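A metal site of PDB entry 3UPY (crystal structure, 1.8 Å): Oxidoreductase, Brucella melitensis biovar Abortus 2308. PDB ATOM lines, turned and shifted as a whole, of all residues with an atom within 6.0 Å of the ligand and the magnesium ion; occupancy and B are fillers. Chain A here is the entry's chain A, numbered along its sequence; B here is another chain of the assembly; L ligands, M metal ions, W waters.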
ATOM      1  N   GLY A 166       5.825 -18.680  27.782  1.00  0.00           N
ATOM      2  CA  GLY A 166       7.046 -18.410  28.538  1.00  0.00           C
ATOM      3  C   GLY A 166       8.198 -17.866  27.673  1.00  0.00           C
ATOM      4  O   GLY A 166       9.156 -17.314  28.193  1.00  0.00           O
ATOM      5  N   ASP A 167       8.116 -17.998  26.344  1.00  0.00           N
ATOM      6  CA  ASP A 167       9.136 -17.411  25.474  1.00  0.00           C
ATOM      7  C   ASP A 167       8.545 -16.113  24.883  1.00  0.00           C
ATOM      8  O   ASP A 167       7.327 -15.953  24.871  1.00  0.00           O
ATOM      9  CB  ASP A 167       9.485 -18.418  24.378  1.00  0.00           C
ATOM     10  CG  ASP A 167      10.796 -18.158  23.691  1.00  0.00           C
ATOM     11  OD1 ASP A 167      11.647 -17.393  24.120  1.00  0.00           O
ATOM     12  OD2 ASP A 167      10.977 -18.811  22.613  1.00  0.00           O
ATOM     13  N   GLU A 168       9.397 -15.223  24.371  1.00  0.00           N
ATOM     14  CA  GLU A 168       8.937 -13.875  23.977  1.00  0.00           C
ATOM     15  C   GLU A 168       7.756 -13.896  23.033  1.00  0.00           C
ATOM     16  O   GLU A 168       6.802 -13.123  23.214  1.00  0.00           O
ATOM     17  CB  GLU A 168      10.101 -12.995  23.455  1.00  0.00           C
ATOM     18  CG  GLU A 168      11.097 -12.605  24.524  1.00  0.00           C
ATOM     19  CD  GLU A 168      12.320 -13.518  24.545  1.00  0.00           C
ATOM     20  OE1 GLU A 168      12.117 -14.777  24.372  1.00  0.00           O
ATOM     21  OE2 GLU A 168      13.435 -13.013  24.769  1.00  0.00           O
ATOM     22  N   PRO A 169       7.738 -14.800  22.042  1.00  0.00           N
ATOM     23  CA  PRO A 169       6.585 -14.687  21.116  1.00  0.00           C
ATOM     24  C   PRO A 169       5.253 -14.986  21.760  1.00  0.00           C
ATOM     25  O   PRO A 169       4.274 -14.269  21.540  1.00  0.00           O
ATOM     26  CB  PRO A 169       6.869 -15.725  20.009  1.00  0.00           C
ATOM     27  CG  PRO A 169       8.276 -16.119  20.172  1.00  0.00           C
ATOM     28  CD  PRO A 169       8.695 -15.844  21.598  1.00  0.00           C
ATOM     29  N   LYS A 191      10.233  -7.257  21.558  1.00  0.00           N
ATOM     30  CA  LYS A 191      11.034  -7.597  22.737  1.00  0.00           C
ATOM     31  C   LYS A 191      12.198  -6.584  22.845  1.00  0.00           C
ATOM     32  O   LYS A 191      12.435  -5.851  21.875  1.00  0.00           O
ATOM     33  CB  LYS A 191      11.581  -9.013  22.576  1.00  0.00           C
ATOM     34  CG  LYS A 191      12.513  -9.165  21.392  1.00  0.00           C
ATOM     35  CD  LYS A 191      13.110 -10.574  21.225  1.00  0.00           C
ATOM     36  CE  LYS A 191      14.194 -10.858  22.298  1.00  0.00           C
ATOM     37  NZ  LYS A 191      15.098 -12.080  22.103  1.00  0.00           N
ATOM     38  N   GLY A 192      12.880  -6.507  23.968  1.00  0.00           N
ATOM     39  CA  GLY A 192      14.122  -5.661  24.033  1.00  0.00           C
ATOM     40  C   GLY A 192      15.494  -6.401  24.099  1.00  0.00           C
ATOM     41  O   GLY A 192      15.551  -7.568  24.348  1.00  0.00           O
ATOM     42  N   LYS A 193      16.572  -5.668  23.854  1.00  0.00           N
ATOM     43  CA  LYS A 193      17.955  -6.134  24.173  1.00  0.00           C
ATOM     44  C   LYS A 193      18.765  -5.027  24.831  1.00  0.00           C
ATOM     45  O   LYS A 193      18.759  -3.847  24.370  1.00  0.00           O
ATOM     46  CB  LYS A 193      18.684  -6.589  22.917  1.00  0.00           C
ATOM     47  CG  LYS A 193      18.054  -7.795  22.219  1.00  0.00           C
ATOM     48  CD  LYS A 193      18.880  -9.079  22.388  1.00  0.00           C
ATOM     49  CE  LYS A 193      20.008  -9.162  21.347  1.00  0.00           C
ATOM     50  NZ  LYS A 193      20.949 -10.367  21.585  1.00  0.00           N
ATOM     51  N   GLU A 222      23.804 -17.195  18.995  1.00  0.00           N
ATOM     52  CA  GLU A 222      22.582 -16.893  18.243  1.00  0.00           C
ATOM     53  C   GLU A 222      21.746 -15.827  18.958  1.00  0.00           C
ATOM     54  O   GLU A 222      20.925 -15.188  18.339  1.00  0.00           O
ATOM     55  CB  GLU A 222      21.790 -18.171  18.089  1.00  0.00           C
ATOM     56  CG  GLU A 222      21.097 -18.520  19.269  1.00  0.00           C
ATOM     57  CD  GLU A 222      20.071 -19.610  19.156  1.00  0.00           C
ATOM     58  OE1 GLU A 222      19.743 -20.057  20.274  1.00  0.00           O
ATOM     59  OE2 GLU A 222      19.525 -19.943  18.061  1.00  0.00           O
ATOM     60  N   PHE A 223      22.016 -15.658  20.234  1.00  0.00           N
ATOM     61  CA  PHE A 223      21.454 -14.579  20.996  1.00  0.00           C
ATOM     62  C   PHE A 223      22.178 -13.237  20.541  1.00  0.00           C
ATOM     63  O   PHE A 223      21.584 -12.338  20.089  1.00  0.00           O
ATOM     64  CB  PHE A 223      21.567 -14.849  22.547  1.00  0.00           C
ATOM     65  CG  PHE A 223      20.842 -16.155  23.085  1.00  0.00           C
ATOM     66  CD1 PHE A 223      19.925 -16.881  22.341  1.00  0.00           C
ATOM     67  CD2 PHE A 223      21.073 -16.621  24.400  1.00  0.00           C
ATOM     68  CE1 PHE A 223      19.311 -17.983  22.816  1.00  0.00           C
ATOM     69  CE2 PHE A 223      20.428 -17.762  24.915  1.00  0.00           C
ATOM     70  CZ  PHE A 223      19.522 -18.441  24.133  1.00  0.00           C
ATOM     71  N   ILE A 224      23.501 -13.182  20.660  1.00  0.00           N
ATOM     72  CA  ILE A 224      24.304 -12.019  20.335  1.00  0.00           C
ATOM     73  C   ILE A 224      24.266 -11.611  18.858  1.00  0.00           C
ATOM     74  O   ILE A 224      24.299 -10.410  18.529  1.00  0.00           O
ATOM     75  CB  ILE A 224      25.837 -12.274  20.720  1.00  0.00           C
ATOM     76  CG1 ILE A 224      26.071 -12.420  22.228  1.00  0.00           C
ATOM     77  CG2 ILE A 224      26.608 -11.202  20.171  1.00  0.00           C
ATOM     78  CD1 ILE A 224      26.073 -11.043  23.059  1.00  0.00           C
ATOM     79  N   LYS A 228      18.187 -15.353  17.179  1.00  0.00           N
ATOM     80  CA  LYS A 228      17.026 -15.655  17.997  1.00  0.00           C
ATOM     81  C   LYS A 228      15.939 -14.542  17.976  1.00  0.00           C
ATOM     82  O   LYS A 228      14.723 -14.821  17.935  1.00  0.00           O
ATOM     83  CB  LYS A 228      17.479 -15.853  19.428  1.00  0.00           C
ATOM     84  CG  LYS A 228      16.359 -16.256  20.365  1.00  0.00           C
ATOM     85  CD  LYS A 228      15.701 -17.580  19.934  1.00  0.00           C
ATOM     86  CE  LYS A 228      16.371 -18.800  20.394  1.00  0.00           C
ATOM     87  NZ  LYS A 228      15.449 -19.879  19.937  1.00  0.00           N
ATOM     88  N   THR A 229      16.382 -13.293  17.970  1.00  0.00           N
ATOM     89  CA  THR A 229      15.490 -12.169  17.857  1.00  0.00           C
ATOM     90  C   THR A 229      14.698 -12.164  16.533  1.00  0.00           C
ATOM     91  O   THR A 229      13.479 -11.896  16.530  1.00  0.00           O
ATOM     92  CB  THR A 229      16.197 -10.829  18.118  1.00  0.00           C
ATOM     93  OG1 THR A 229      16.605 -10.810  19.514  1.00  0.00           O
ATOM     94  CG2 THR A 229      15.286  -9.639  17.825  1.00  0.00           C
ATOM     95  N   GLU A 232      12.094 -15.067  16.788  1.00  0.00           N
ATOM     96  CA  GLU A 232      11.000 -14.762  17.736  1.00  0.00           C
ATOM     97  C   GLU A 232      10.049 -13.713  17.163  1.00  0.00           C
ATOM     98  O   GLU A 232       8.807 -13.822  17.304  1.00  0.00           O
ATOM     99  CB  GLU A 232      11.546 -14.273  19.062  1.00  0.00           C
ATOM    100  CG  GLU A 232      12.043 -15.458  19.867  1.00  0.00           C
ATOM    101  CD  GLU A 232      12.746 -15.098  21.184  1.00  0.00           C
ATOM    102  OE1 GLU A 232      12.954 -13.929  21.520  1.00  0.00           O
ATOM    103  OE2 GLU A 232      13.138 -16.051  21.883  1.00  0.00           O
ATOM    104  N   HIS A 323       9.323 -13.089  31.394  1.00  0.00           N
ATOM    105  CA  HIS A 323       8.894 -14.283  30.626  1.00  0.00           C
ATOM    106  C   HIS A 323       9.717 -15.401  31.329  1.00  0.00           C
ATOM    107  O   HIS A 323      10.847 -15.150  31.566  1.00  0.00           O
ATOM    108  CB  HIS A 323       9.193 -14.131  29.102  1.00  0.00           C
ATOM    109  CG  HIS A 323      10.656 -14.174  28.712  1.00  0.00           C
ATOM    110  ND1 HIS A 323      11.552 -13.163  28.994  1.00  0.00           N
ATOM    111  CD2 HIS A 323      11.356 -15.113  28.036  1.00  0.00           C
ATOM    112  CE1 HIS A 323      12.743 -13.485  28.512  1.00  0.00           C
ATOM    113  NE2 HIS A 323      12.642 -14.674  27.917  1.00  0.00           N
ATOM    114  N   THR A 325      10.455 -18.595  30.328  1.00  0.00           N
ATOM    115  CA  THR A 325      10.875 -19.644  29.401  1.00  0.00           C
ATOM    116  C   THR A 325      10.164 -20.969  29.716  1.00  0.00           C
ATOM    117  O   THR A 325       8.918 -20.998  29.858  1.00  0.00           O
ATOM    118  CB  THR A 325      12.424 -19.756  29.297  1.00  0.00           C
ATOM    119  OG1 THR A 325      12.982 -20.245  30.547  1.00  0.00           O
ATOM    120  CG2 THR A 325      13.019 -18.375  28.930  1.00  0.00           C
ATOM    121  N   LEU B 308      17.688 -15.264  33.786  1.00  0.00           N
ATOM    122  CA  LEU B 308      16.777 -14.413  33.024  1.00  0.00           C
ATOM    123  C   LEU B 308      16.752 -12.960  33.532  1.00  0.00           C
ATOM    124  O   LEU B 308      16.119 -12.113  32.907  1.00  0.00           O
ATOM    125  CB  LEU B 308      15.374 -14.997  33.046  1.00  0.00           C
ATOM    126  CG  LEU B 308      15.230 -16.328  32.283  1.00  0.00           C
ATOM    127  CD1 LEU B 308      13.971 -17.053  32.657  1.00  0.00           C
ATOM    128  CD2 LEU B 308      15.237 -16.005  30.815  1.00  0.00           C
HETATM  129  O1  LIG L   1      14.887 -15.012  24.020  1.00  0.00           O
HETATM  130  N1  LIG L   1      15.344 -15.345  25.143  1.00  0.00           N
HETATM  131  C1  LIG L   1      14.727 -16.071  26.035  1.00  0.00           C
HETATM  132  O2  LIG L   1      13.655 -16.608  25.763  1.00  0.00           O
HETATM  133  C2  LIG L   1      16.662 -14.924  25.530  1.00  0.00           C
HETATM  134  C3  LIG L   1      17.613 -15.078  24.378  1.00  0.00           C
HETATM  135  C4  LIG L   1      18.552 -13.898  24.470  1.00  0.00           C
HETATM  136  P1  LIG L   1      18.100 -12.590  23.327  1.00  0.00           P
HETATM  137  O3  LIG L   1      17.783 -13.102  21.892  1.00  0.00           O
HETATM  138  O4  LIG L   1      16.849 -12.020  24.061  1.00  0.00           O
HETATM  139  O5  LIG L   1      19.417 -11.774  23.460  1.00  0.00           O
HETATM  140 MG    MG M   1      13.329 -16.276  23.917  1.00  0.00          MG
HETATM  141  O   HOH W   1      14.674 -17.814  23.635  1.00  0.00           O
HETATM  142  O   HOH W   2      13.426 -19.746  25.376  1.00  0.00           O
HETATM  143  O   HOH W   3      18.962 -12.538  19.433  1.00  0.00           O
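Water W3 lies within hydrogen-bond range of O of Phe 223, O3 of the ligand, OG1 of Thr 229 and O of Glu 222.
The side-chain amino group (NZ) of Lys 191 is in salt-bridge range of the side-chain carboxylate (OE1) of Glu 232 (2.9 Å).
The side-chain amino group of Lys 191 lies within hydrogen-bond range of the side-chain hydroxyl of Thr 229.
The backbone NH of Thr 325 is in hydrogen-bond range of the backbone carbonyl oxygen of Gly 166 (2.8 Å).
NZ of Lys 193 is in hydrogen-bond range of O of Phe 223 (2.6 Å).
OE2 of Glu 168 lies within salt-bridge range of NZ of Lys 191, 3.3 Å away.
The backbone NH (N) of Lys 228 is in hydrogen-bond range of the backbone carbonyl oxygen (O) of Glu 222.
Of the 16 residues printed, 3 come within 4 Å of the magnesium ion.
Residues that only touch the ligand: Phe 223, Lys 228, Thr 229 and Thr 325.
The nearest printed residue that does not touch the ligand is Gly 192 (4.6 Å).
An oxygen (O5) of the ligand lies within salt-bridge range of the side-chain amino group (NZ) of Lys 193, at 2.8 Å.
A ring nitrogen (NE2) of His 323 sits close to an oxygen (O2) of the ligand (3.1 Å).
An oxygen (O4) of the ligand is in salt-bridge range of the side-chain amino group (NZ) of Lys 191 (2.6 Å).
The magnesium ion is bound by an oxygen (O2) of the ligand, at 1.9 Å.
The side-chain carboxylate (OE1) of Glu 168 binds the magnesium ion (2.0 Å).
An oxygen (O1) of the ligand binds the magnesium ion, at 2.0 Å.
The side-chain carboxylate (OD1) of Asp 167 binds the magnesium ion (2.0 Å).
The side-chain carboxylate (OE2) of Glu 232 is bound to the magnesium ion.
The magnesium ion is bound by water W1.
The magnesium ion has six donor atoms within binding distance.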
